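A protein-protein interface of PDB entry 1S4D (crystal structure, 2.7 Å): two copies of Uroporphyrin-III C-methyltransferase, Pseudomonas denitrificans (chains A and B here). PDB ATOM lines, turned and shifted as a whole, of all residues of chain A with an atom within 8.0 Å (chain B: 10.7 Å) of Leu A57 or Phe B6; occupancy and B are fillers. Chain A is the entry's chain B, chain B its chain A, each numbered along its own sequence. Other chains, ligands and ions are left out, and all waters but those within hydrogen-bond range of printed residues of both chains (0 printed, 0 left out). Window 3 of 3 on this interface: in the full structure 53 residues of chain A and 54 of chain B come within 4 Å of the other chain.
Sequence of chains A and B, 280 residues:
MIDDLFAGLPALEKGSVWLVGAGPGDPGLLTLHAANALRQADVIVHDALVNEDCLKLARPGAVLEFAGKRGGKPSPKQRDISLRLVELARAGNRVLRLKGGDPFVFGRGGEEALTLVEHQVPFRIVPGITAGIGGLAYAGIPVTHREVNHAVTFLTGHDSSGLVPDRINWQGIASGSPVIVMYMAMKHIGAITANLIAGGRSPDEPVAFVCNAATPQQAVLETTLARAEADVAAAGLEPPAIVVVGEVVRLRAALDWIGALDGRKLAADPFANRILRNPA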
ATOM      1  N   PHE A   6     -20.999  25.131   1.872  1.00  0.00           N
ATOM      2  CA  PHE A   6     -20.145  26.123   2.546  1.00  0.00           C
ATOM      3  C   PHE A   6     -18.706  25.549   2.528  1.00  0.00           C
ATOM      4  O   PHE A   6     -18.065  25.306   3.539  1.00  0.00           O
ATOM      5  CB  PHE A   6     -20.759  26.603   3.892  1.00  0.00           C
ATOM      6  CG  PHE A   6     -20.307  25.867   5.141  1.00  0.00           C
ATOM      7  CD1 PHE A   6     -19.851  24.562   5.109  1.00  0.00           C
ATOM      8  CD2 PHE A   6     -20.403  26.514   6.383  1.00  0.00           C
ATOM      9  CE1 PHE A   6     -19.451  23.928   6.287  1.00  0.00           C
ATOM     10  CE2 PHE A   6     -20.025  25.895   7.559  1.00  0.00           C
ATOM     11  CZ  PHE A   6     -19.547  24.602   7.518  1.00  0.00           C
ATOM     12  N   PRO A  27     -26.109  30.232  19.724  1.00  0.00           N
ATOM     13  CA  PRO A  27     -25.402  29.487  18.660  1.00  0.00           C
ATOM     14  C   PRO A  27     -25.616  30.082  17.264  1.00  0.00           C
ATOM     15  O   PRO A  27     -24.762  29.860  16.423  1.00  0.00           O
ATOM     16  CB  PRO A  27     -26.009  28.082  18.714  1.00  0.00           C
ATOM     17  CG  PRO A  27     -26.729  28.023  19.990  1.00  0.00           C
ATOM     18  CD  PRO A  27     -27.140  29.413  20.386  1.00  0.00           C
ATOM     19  N   LEU A  30     -22.564  32.215  15.933  1.00  0.00           N
ATOM     20  CA  LEU A  30     -21.379  31.603  15.354  1.00  0.00           C
ATOM     21  C   LEU A  30     -21.228  32.105  13.916  1.00  0.00           C
ATOM     22  O   LEU A  30     -22.238  32.332  13.234  1.00  0.00           O
ATOM     23  CB  LEU A  30     -21.568  30.095  15.328  1.00  0.00           C
ATOM     24  CG  LEU A  30     -21.013  29.174  16.412  1.00  0.00           C
ATOM     25  CD1 LEU A  30     -20.485  29.930  17.628  1.00  0.00           C
ATOM     26  CD2 LEU A  30     -22.041  28.133  16.798  1.00  0.00           C
ATOM     27  N   THR A  31     -19.998  32.299  13.451  1.00  0.00           N
ATOM     28  CA  THR A  31     -19.752  32.598  12.036  1.00  0.00           C
ATOM     29  C   THR A  31     -19.653  31.303  11.262  1.00  0.00           C
ATOM     30  O   THR A  31     -19.366  30.273  11.854  1.00  0.00           O
ATOM     31  CB  THR A  31     -18.412  33.318  11.845  1.00  0.00           C
ATOM     32  OG1 THR A  31     -17.341  32.495  12.358  1.00  0.00           O
ATOM     33  CG2 THR A  31     -18.346  34.643  12.643  1.00  0.00           C
ATOM     34  N   LEU A  32     -19.845  31.352   9.938  1.00  0.00           N
ATOM     35  CA  LEU A  32     -19.679  30.169   9.073  1.00  0.00           C
ATOM     36  C   LEU A  32     -18.322  29.471   9.345  1.00  0.00           C
ATOM     37  O   LEU A  32     -18.263  28.247   9.558  1.00  0.00           O
ATOM     38  CB  LEU A  32     -19.827  30.548   7.600  1.00  0.00           C
ATOM     39  CG  LEU A  32     -21.243  30.649   6.981  1.00  0.00           C
ATOM     40  CD1 LEU A  32     -22.305  31.076   7.978  1.00  0.00           C
ATOM     41  CD2 LEU A  32     -21.331  31.558   5.724  1.00  0.00           C
ATOM     42  N   ALA A  34     -16.468  29.596  12.111  1.00  0.00           N
ATOM     43  CA  ALA A  34     -16.490  28.956  13.418  1.00  0.00           C
ATOM     44  C   ALA A  34     -17.217  27.614  13.340  1.00  0.00           C
ATOM     45  O   ALA A  34     -16.680  26.591  13.788  1.00  0.00           O
ATOM     46  CB  ALA A  34     -17.130  29.871  14.453  1.00  0.00           C
ATOM     47  N   ALA A  35     -18.422  27.621  12.758  1.00  0.00           N
ATOM     48  CA  ALA A  35     -19.216  26.395  12.551  1.00  0.00           C
ATOM     49  C   ALA A  35     -18.434  25.373  11.716  1.00  0.00           C
ATOM     50  O   ALA A  35     -18.397  24.183  12.021  1.00  0.00           O
ATOM     51  CB  ALA A  35     -20.532  26.731  11.878  1.00  0.00           C
ATOM     52  N   ASN A  36     -17.781  25.858  10.666  1.00  0.00           N
ATOM     53  CA  ASN A  36     -16.858  25.020   9.920  1.00  0.00           C
ATOM     54  C   ASN A  36     -15.698  24.457  10.773  1.00  0.00           C
ATOM     55  O   ASN A  36     -15.433  23.263  10.709  1.00  0.00           O
ATOM     56  CB  ASN A  36     -16.364  25.721   8.651  1.00  0.00           C
ATOM     57  CG  ASN A  36     -15.826  24.742   7.639  1.00  0.00           C
ATOM     58  OD1 ASN A  36     -16.391  23.663   7.436  1.00  0.00           O
ATOM     59  ND2 ASN A  36     -14.710  25.090   7.022  1.00  0.00           N
ATOM     60  N   ALA A  37     -15.035  25.285  11.579  1.00  0.00           N
ATOM     61  CA  ALA A  37     -14.007  24.771  12.510  1.00  0.00           C
ATOM     62  C   ALA A  37     -14.552  23.659  13.411  1.00  0.00           C
ATOM     63  O   ALA A  37     -14.026  22.545  13.428  1.00  0.00           O
ATOM     64  CB  ALA A  37     -13.422  25.881  13.355  1.00  0.00           C
ATOM     65  N   LEU A  38     -15.624  23.968  14.137  1.00  0.00           N
ATOM     66  CA  LEU A  38     -16.274  23.021  15.038  1.00  0.00           C
ATOM     67  C   LEU A  38     -16.465  21.635  14.419  1.00  0.00           C
ATOM     68  O   LEU A  38     -16.227  20.624  15.078  1.00  0.00           O
ATOM     69  CB  LEU A  38     -17.618  23.582  15.474  1.00  0.00           C
ATOM     70  CG  LEU A  38     -17.789  24.155  16.883  1.00  0.00           C
ATOM     71  CD1 LEU A  38     -16.507  24.121  17.680  1.00  0.00           C
ATOM     72  CD2 LEU A  38     -18.400  25.572  16.849  1.00  0.00           C
ATOM     73  N   ARG A  39     -16.874  21.601  13.149  1.00  0.00           N
ATOM     74  CA  ARG A  39     -17.226  20.353  12.478  1.00  0.00           C
ATOM     75  C   ARG A  39     -15.986  19.559  12.094  1.00  0.00           C
ATOM     76  O   ARG A  39     -16.066  18.364  11.864  1.00  0.00           O
ATOM     77  CB  ARG A  39     -18.207  20.603  11.297  1.00  0.00           C
ATOM     78  CG  ARG A  39     -17.728  20.249   9.877  1.00  0.00           C
ATOM     79  CD  ARG A  39     -18.491  20.945   8.730  1.00  0.00           C
ATOM     80  NE  ARG A  39     -19.953  20.841   8.872  1.00  0.00           N
ATOM     81  CZ  ARG A  39     -20.727  19.890   8.316  1.00  0.00           C
ATOM     82  NH1 ARG A  39     -20.207  18.918   7.558  1.00  0.00           N
ATOM     83  NH2 ARG A  39     -22.039  19.909   8.526  1.00  0.00           N
ATOM     84  N   GLN A  40     -14.837  20.223  12.077  1.00  0.00           N
ATOM     85  CA  GLN A  40     -13.582  19.600  11.649  1.00  0.00           C
ATOM     86  C   GLN A  40     -12.660  19.225  12.800  1.00  0.00           C
ATOM     87  O   GLN A  40     -11.827  18.330  12.659  1.00  0.00           O
ATOM     88  CB  GLN A  40     -12.821  20.528  10.713  1.00  0.00           C
ATOM     89  CG  GLN A  40     -13.243  20.411   9.282  1.00  0.00           C
ATOM     90  CD  GLN A  40     -12.660  21.501   8.402  1.00  0.00           C
ATOM     91  OE1 GLN A  40     -13.401  22.266   7.809  1.00  0.00           O
ATOM     92  NE2 GLN A  40     -11.341  21.569   8.312  1.00  0.00           N
ATOM     93  N   ALA A  41     -12.799  19.916  13.931  1.00  0.00           N
ATOM     94  CA  ALA A  41     -11.841  19.797  15.029  1.00  0.00           C
ATOM     95  C   ALA A  41     -11.637  18.382  15.593  1.00  0.00           C
ATOM     96  O   ALA A  41     -12.579  17.610  15.749  1.00  0.00           O
ATOM     97  CB  ALA A  41     -12.198  20.744  16.125  1.00  0.00           C
ATOM     98  N   ILE A  44     -11.468  20.391  20.986  1.00  0.00           N
ATOM     99  CA  ILE A  44     -12.047  21.713  21.181  1.00  0.00           C
ATOM    100  C   ILE A  44     -11.753  22.107  22.613  1.00  0.00           C
ATOM    101  O   ILE A  44     -12.346  21.552  23.566  1.00  0.00           O
ATOM    102  CB  ILE A  44     -13.572  21.684  20.919  1.00  0.00           C
ATOM    103  CG1 ILE A  44     -13.846  21.325  19.462  1.00  0.00           C
ATOM    104  CG2 ILE A  44     -14.221  23.030  21.245  1.00  0.00           C
ATOM    105  CD1 ILE A  44     -15.267  21.041  19.173  1.00  0.00           C
ATOM    106  N   GLU A  52     -22.926  24.795  25.919  1.00  0.00           N
ATOM    107  CA  GLU A  52     -23.251  23.552  25.207  1.00  0.00           C
ATOM    108  C   GLU A  52     -23.526  23.799  23.726  1.00  0.00           C
ATOM    109  O   GLU A  52     -22.655  23.585  22.901  1.00  0.00           O
ATOM    110  CB  GLU A  52     -24.449  22.816  25.848  1.00  0.00           C
ATOM    111  CG  GLU A  52     -24.790  21.465  25.202  1.00  0.00           C
ATOM    112  CD  GLU A  52     -26.106  20.863  25.701  1.00  0.00           C
ATOM    113  OE1 GLU A  52     -26.427  21.015  26.903  1.00  0.00           O
ATOM    114  OE2 GLU A  52     -26.822  20.220  24.891  1.00  0.00           O
ATOM    115  N   ASP A  53     -24.702  24.319  23.407  1.00  0.00           N
ATOM    116  CA  ASP A  53     -25.252  24.319  22.045  1.00  0.00           C
ATOM    117  C   ASP A  53     -24.201  24.372  20.930  1.00  0.00           C
ATOM    118  O   ASP A  53     -24.198  23.510  20.043  1.00  0.00           O
ATOM    119  CB  ASP A  53     -26.304  25.430  21.871  1.00  0.00           C
ATOM    120  CG  ASP A  53     -27.036  25.783  23.180  1.00  0.00           C
ATOM    121  OD1 ASP A  53     -28.059  25.097  23.499  1.00  0.00           O
ATOM    122  OD2 ASP A  53     -26.645  26.731  23.934  1.00  0.00           O
ATOM    123  N   CYS A  54     -23.271  25.312  20.974  1.00  0.00           N
ATOM    124  CA  CYS A  54     -22.106  25.355  20.083  1.00  0.00           C
ATOM    125  C   CYS A  54     -21.405  24.007  19.935  1.00  0.00           C
ATOM    126  O   CYS A  54     -21.166  23.545  18.823  1.00  0.00           O
ATOM    127  CB  CYS A  54     -21.099  26.365  20.604  1.00  0.00           C
ATOM    128  SG  CYS A  54     -21.791  28.024  20.660  1.00  0.00           S
ATOM    129  N   LEU A  55     -21.081  23.395  21.073  1.00  0.00           N
ATOM    130  CA  LEU A  55     -20.282  22.174  21.141  1.00  0.00           C
ATOM    131  C   LEU A  55     -20.922  20.990  20.447  1.00  0.00           C
ATOM    132  O   LEU A  55     -20.223  20.085  20.018  1.00  0.00           O
ATOM    133  CB  LEU A  55     -19.946  21.829  22.594  1.00  0.00           C
ATOM    134  CG  LEU A  55     -19.113  22.875  23.353  1.00  0.00           C
ATOM    135  CD1 LEU A  55     -18.880  22.495  24.843  1.00  0.00           C
ATOM    136  CD2 LEU A  55     -17.791  23.115  22.639  1.00  0.00           C
ATOM    137  N   LYS A  56     -22.249  21.023  20.326  1.00  0.00           N
ATOM    138  CA  LYS A  56     -23.026  19.992  19.636  1.00  0.00           C
ATOM    139  C   LYS A  56     -22.691  19.863  18.146  1.00  0.00           C
ATOM    140  O   LYS A  56     -23.074  18.884  17.513  1.00  0.00           O
ATOM    141  CB  LYS A  56     -24.534  20.259  19.811  1.00  0.00           C
ATOM    142  CG  LYS A  56     -25.335  19.140  20.505  1.00  0.00           C
ATOM    143  CD  LYS A  56     -25.986  18.185  19.487  1.00  0.00           C
ATOM    144  CE  LYS A  56     -27.513  18.124  19.640  1.00  0.00           C
ATOM    145  NZ  LYS A  56     -27.990  16.722  19.813  1.00  0.00           N
ATOM    146  N   LEU A  57     -21.979  20.839  17.594  1.00  0.00           N
ATOM    147  CA  LEU A  57     -21.601  20.817  16.184  1.00  0.00           C
ATOM    148  C   LEU A  57     -20.350  19.970  15.932  1.00  0.00           C
ATOM    149  O   LEU A  57     -20.090  19.529  14.786  1.00  0.00           O
ATOM    150  CB  LEU A  57     -21.388  22.236  15.655  1.00  0.00           C
ATOM    151  CG  LEU A  57     -22.603  23.089  15.281  1.00  0.00           C
ATOM    152  CD1 LEU A  57     -22.171  24.495  14.964  1.00  0.00           C
ATOM    153  CD2 LEU A  57     -23.350  22.518  14.094  1.00  0.00           C
ATOM    154  N   ALA A  58     -19.575  19.751  17.000  1.00  0.00           N
ATOM    155  CA  ALA A  58     -18.373  18.918  16.946  1.00  0.00           C
ATOM    156  C   ALA A  58     -18.719  17.569  16.356  1.00  0.00           C
ATOM    157  O   ALA A  58     -19.802  17.049  16.610  1.00  0.00           O
ATOM    158  CB  ALA A  58     -17.797  18.745  18.327  1.00  0.00           C
ATOM    159  N   ARG A  59     -17.817  17.017  15.548  1.00  0.00           N
ATOM    160  CA  ARG A  59     -17.999  15.659  15.037  1.00  0.00           C
ATOM    161  C   ARG A  59     -17.954  14.689  16.222  1.00  0.00           C
ATOM    162  O   ARG A  59     -17.393  15.024  17.272  1.00  0.00           O
ATOM    163  CB  ARG A  59     -16.960  15.307  13.954  1.00  0.00           C
ATOM    164  CG  ARG A  59     -15.496  15.504  14.340  1.00  0.00           C
ATOM    165  CD  ARG A  59     -14.534  14.447  13.787  1.00  0.00           C
ATOM    166  NE  ARG A  59     -13.296  15.044  13.273  1.00  0.00           N
ATOM    167  CZ  ARG A  59     -12.910  15.021  11.994  1.00  0.00           C
ATOM    168  NH1 ARG A  59     -13.661  14.410  11.073  1.00  0.00           N
ATOM    169  NH2 ARG A  59     -11.767  15.609  11.634  1.00  0.00           N
ATOM    170  N   PRO A  60     -18.566  13.512  16.091  1.00  0.00           N
ATOM    171  CA  PRO A  60     -18.536  12.540  17.195  1.00  0.00           C
ATOM    172  C   PRO A  60     -17.120  11.980  17.329  1.00  0.00           C
ATOM    173  O   PRO A  60     -16.437  11.724  16.310  1.00  0.00           O
ATOM    174  CB  PRO A  60     -19.533  11.447  16.759  1.00  0.00           C
ATOM    175  CG  PRO A  60     -20.255  12.006  15.559  1.00  0.00           C
ATOM    176  CD  PRO A  60     -19.307  12.991  14.923  1.00  0.00           C
ATOM    177  N   ALA A  62     -14.741  13.788  18.632  1.00  0.00           N
ATOM    178  CA  ALA A  62     -13.901  14.945  18.932  1.00  0.00           C
ATOM    179  C   ALA A  62     -13.794  15.013  20.443  1.00  0.00           C
ATOM    180  O   ALA A  62     -14.740  14.661  21.132  1.00  0.00           O
ATOM    181  CB  ALA A  62     -14.533  16.227  18.403  1.00  0.00           C
ATOM    182  N   LEU A  64     -13.631  17.271  23.919  1.00  0.00           N
ATOM    183  CA  LEU A  64     -14.005  18.577  24.423  1.00  0.00           C
ATOM    184  C   LEU A  64     -13.272  18.788  25.726  1.00  0.00           C
ATOM    185  O   LEU A  64     -13.452  18.024  26.651  1.00  0.00           O
ATOM    186  CB  LEU A  64     -15.521  18.665  24.637  1.00  0.00           C
ATOM    187  CG  LEU A  64     -16.484  18.061  23.591  1.00  0.00           C
ATOM    188  CD1 LEU A  64     -17.947  18.294  24.009  1.00  0.00           C
ATOM    189  CD2 LEU A  64     -16.228  18.563  22.152  1.00  0.00           C
ATOM    190  N   PHE B   6     -28.157  21.298  10.005  1.00  0.00           N
ATOM    191  CA  PHE B   6     -27.807  22.100  11.239  1.00  0.00           C
ATOM    192  C   PHE B   6     -28.191  23.583  11.204  1.00  0.00           C
ATOM    193  O   PHE B   6     -27.363  24.478  10.936  1.00  0.00           O
ATOM    194  CB  PHE B   6     -26.368  21.822  11.704  1.00  0.00           C
ATOM    195  CG  PHE B   6     -26.258  20.628  12.630  1.00  0.00           C
ATOM    196  CD1 PHE B   6     -26.885  20.646  13.887  1.00  0.00           C
ATOM    197  CD2 PHE B   6     -25.562  19.479  12.244  1.00  0.00           C
ATOM    198  CE1 PHE B   6     -26.803  19.550  14.754  1.00  0.00           C
ATOM    199  CE2 PHE B   6     -25.473  18.372  13.102  1.00  0.00           C
ATOM    200  CZ  PHE B   6     -26.092  18.409  14.362  1.00  0.00           C
ATOM    201  N   ALA B   7     -29.481  23.789  11.479  1.00  0.00           N
ATOM    202  CA  ALA B   7     -30.165  25.073  11.542  1.00  0.00           C
ATOM    203  C   ALA B   7     -31.607  24.861  12.065  1.00  0.00           C
ATOM    204  O   ALA B   7     -32.530  24.622  11.281  1.00  0.00           O
ATOM    205  CB  ALA B   7     -30.169  25.761  10.173  1.00  0.00           C
ATOM    206  N   GLY B   8     -31.806  24.893  13.393  1.00  0.00           N
ATOM    207  CA  GLY B   8     -33.154  24.986  13.990  1.00  0.00           C
ATOM    208  C   GLY B   8     -33.203  26.354  14.681  1.00  0.00           C
ATOM    209  O   GLY B   8     -32.991  26.438  15.901  1.00  0.00           O
ATOM    210  N   LEU B   9     -33.304  27.425  13.889  1.00  0.00           N
ATOM    211  CA  LEU B   9     -33.169  28.788  14.402  1.00  0.00           C
ATOM    212  C   LEU B   9     -34.336  29.633  13.933  1.00  0.00           C
ATOM    213  O   LEU B   9     -35.116  29.217  13.068  1.00  0.00           O
ATOM    214  CB  LEU B   9     -31.819  29.432  14.030  1.00  0.00           C
ATOM    215  CG  LEU B   9     -31.106  29.289  12.686  1.00  0.00           C
ATOM    216  CD1 LEU B   9     -29.843  30.118  12.638  1.00  0.00           C
ATOM    217  CD2 LEU B   9     -30.672  27.889  12.571  1.00  0.00           C
ATOM    218  N   PRO B  10     -34.510  30.828  14.497  1.00  0.00           N
ATOM    219  CA  PRO B  10     -35.758  31.532  14.180  1.00  0.00           C
ATOM    220  C   PRO B  10     -35.941  31.824  12.693  1.00  0.00           C
ATOM    221  O   PRO B  10     -34.969  32.030  11.964  1.00  0.00           O
ATOM    222  CB  PRO B  10     -35.686  32.801  15.050  1.00  0.00           C
ATOM    223  CG  PRO B  10     -34.744  32.408  16.142  1.00  0.00           C
ATOM    224  CD  PRO B  10     -33.669  31.622  15.428  1.00  0.00           C
ATOM    225  N   THR B  31     -22.729  35.404  10.246  1.00  0.00           N
ATOM    226  CA  THR B  31     -23.246  34.566  11.324  1.00  0.00           C
ATOM    227  C   THR B  31     -24.245  33.582  10.736  1.00  0.00           C
ATOM    228  O   THR B  31     -24.786  33.804   9.645  1.00  0.00           O
ATOM    229  CB  THR B  31     -23.933  35.403  12.403  1.00  0.00           C
ATOM    230  OG1 THR B  31     -24.911  36.255  11.787  1.00  0.00           O
ATOM    231  CG2 THR B  31     -22.953  36.353  13.072  1.00  0.00           C
ATOM    232  N   LEU B  32     -24.478  32.490  11.458  1.00  0.00           N
ATOM    233  CA  LEU B  32     -25.413  31.478  11.020  1.00  0.00           C
ATOM    234  C   LEU B  32     -26.784  32.113  10.919  1.00  0.00           C
ATOM    235  O   LEU B  32     -27.544  31.820   9.998  1.00  0.00           O
ATOM    236  CB  LEU B  32     -25.431  30.310  11.980  1.00  0.00           C
ATOM    237  CG  LEU B  32     -24.152  29.468  12.010  1.00  0.00           C
ATOM    238  CD1 LEU B  32     -24.302  28.321  13.052  1.00  0.00           C
ATOM    239  CD2 LEU B  32     -23.854  28.913  10.625  1.00  0.00           C
ATOM    240  N   HIS B  33     -27.079  33.032  11.835  1.00  0.00           N
ATOM    241  CA  HIS B  33     -28.321  33.806  11.738  1.00  0.00           C
ATOM    242  C   HIS B  33     -28.415  34.557  10.405  1.00  0.00           C
ATOM    243  O   HIS B  33     -29.466  34.571   9.784  1.00  0.00           O
ATOM    244  CB  HIS B  33     -28.437  34.783  12.910  1.00  0.00           C
ATOM    245  CG  HIS B  33     -29.086  34.200  14.129  1.00  0.00           C
ATOM    246  ND1 HIS B  33     -28.672  34.509  15.410  1.00  0.00           N
ATOM    247  CD2 HIS B  33     -30.128  33.344  14.262  1.00  0.00           C
ATOM    248  CE1 HIS B  33     -29.428  33.865  16.280  1.00  0.00           C
ATOM    249  NE2 HIS B  33     -30.322  33.157  15.612  1.00  0.00           N
ATOM    250  N   ALA B  35     -26.772  33.800   7.552  1.00  0.00           N
ATOM    251  CA  ALA B  35     -26.837  32.852   6.439  1.00  0.00           C
ATOM    252  C   ALA B  35     -28.272  32.394   6.271  1.00  0.00           C
ATOM    253  O   ALA B  35     -28.807  32.389   5.162  1.00  0.00           O
ATOM    254  CB  ALA B  35     -25.911  31.665   6.675  1.00  0.00           C
ATOM    255  N   ASN B  36     -28.889  32.040   7.394  1.00  0.00           N
ATOM    256  CA  ASN B  36     -30.280  31.640   7.437  1.00  0.00           C
ATOM    257  C   ASN B  36     -31.235  32.724   6.907  1.00  0.00           C
ATOM    258  O   ASN B  36     -32.116  32.426   6.092  1.00  0.00           O
ATOM    259  CB  ASN B  36     -30.671  31.183   8.851  1.00  0.00           C
ATOM    260  CG  ASN B  36     -31.829  30.197   8.836  1.00  0.00           C
ATOM    261  OD1 ASN B  36     -31.716  29.094   8.286  1.00  0.00           O
ATOM    262  ND2 ASN B  36     -32.970  30.605   9.398  1.00  0.00           N
ATOM    263  N   ARG B  39     -30.993  33.009   3.325  1.00  0.00           N
ATOM    264  CA  ARG B  39     -31.706  31.899   2.691  1.00  0.00           C
ATOM    265  C   ARG B  39     -33.191  32.168   2.584  1.00  0.00           C
ATOM    266  O   ARG B  39     -33.820  31.686   1.656  1.00  0.00           O
ATOM    267  CB  ARG B  39     -31.498  30.565   3.431  1.00  0.00           C
ATOM    268  CG  ARG B  39     -31.482  29.327   2.513  1.00  0.00           C
ATOM    269  CD  ARG B  39     -32.889  28.757   2.073  1.00  0.00           C
ATOM    270  NE  ARG B  39     -33.060  28.326   0.658  1.00  0.00           N
ATOM    271  CZ  ARG B  39     -32.159  28.421  -0.342  1.00  0.00           C
ATOM    272  NH1 ARG B  39     -32.486  27.985  -1.556  1.00  0.00           N
ATOM    273  NH2 ARG B  39     -30.940  28.930  -0.153  1.00  0.00           N
ATOM    274  N   GLN B  40     -33.774  32.911   3.521  1.00  0.00           N
ATOM    275  CA  GLN B  40     -35.231  33.028   3.497  1.00  0.00           C
ATOM    276  C   GLN B  40     -35.865  34.385   3.171  1.00  0.00           C
ATOM    277  O   GLN B  40     -37.077  34.461   3.000  1.00  0.00           O
ATOM    278  CB  GLN B  40     -35.889  32.352   4.708  1.00  0.00           C
ATOM    279  CG  GLN B  40     -35.309  32.689   6.047  1.00  0.00           C
ATOM    280  CD  GLN B  40     -35.695  31.679   7.102  1.00  0.00           C
ATOM    281  OE1 GLN B  40     -34.966  30.726   7.339  1.00  0.00           O
ATOM    282  NE2 GLN B  40     -36.834  31.881   7.731  1.00  0.00           N
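Printed residues of chain B within 4 Å of Pro A27: Leu B32 (3.7 Å). Of the printed residues of chain B, Leu A30 touches Thr B31 (3.1 Å) and Leu B32 (2.9 Å). Of the printed residues of chain B, Leu A32 touches Leu B32 and Ala B35. No residue of chain B comes within 4 Å of Ala A35. Leu A38 touches none of the printed residues of chain B. Glu A52 touches none of the printed residues of chain B. Leu A57 touches just one residue of chain B: Phe B6. No residue of chain B comes within 4 Å of Ala A58. Leu A64 touches none of the printed residues of chain B. Of chain A, only Leu A57 comes within 4 Å of Phe B6. Of the printed residues of chain A, Leu B32 touches Pro A27 (3.7 Å), Leu A30 (2.9 Å) and Leu A32 (3.8 Å). Of the printed residues of chain A, Ala B35 touches Leu A32.
Among the printed residues, merely in contact across the chains: Pro A27 with Leu B32 (3.7 Å), Leu A30 with Thr B31 (3.1 Å), Leu A32 with Leu B32 (3.8 Å), Leu A32 with Ala B35 (3.9 Å) and Leu A57 with Phe B6 (3.8 Å).
N of Leu B32 sits at hydrogen-bond distance from O of Leu A30, 2.9 Å away.
Leu A32 touches its own counterpart, Leu B32. Leu A32 touches Ala B35, but with the chains exchanged Ala A35 does not touch Leu B32 (4.2 Å). Of the 6 pairs that touch across the chains among the printed residues, 1 has its exchanged pair printed and touching as well.
Of the 12 printed residues of chain B, 4 touch a printed residue of chain A. Hydrophobic or aromatic side chains of chain B that line the printed part of chain A: Phe B6, Leu B32 and Ala B35. Among the printed residues, 6 pairs touch across the chains.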
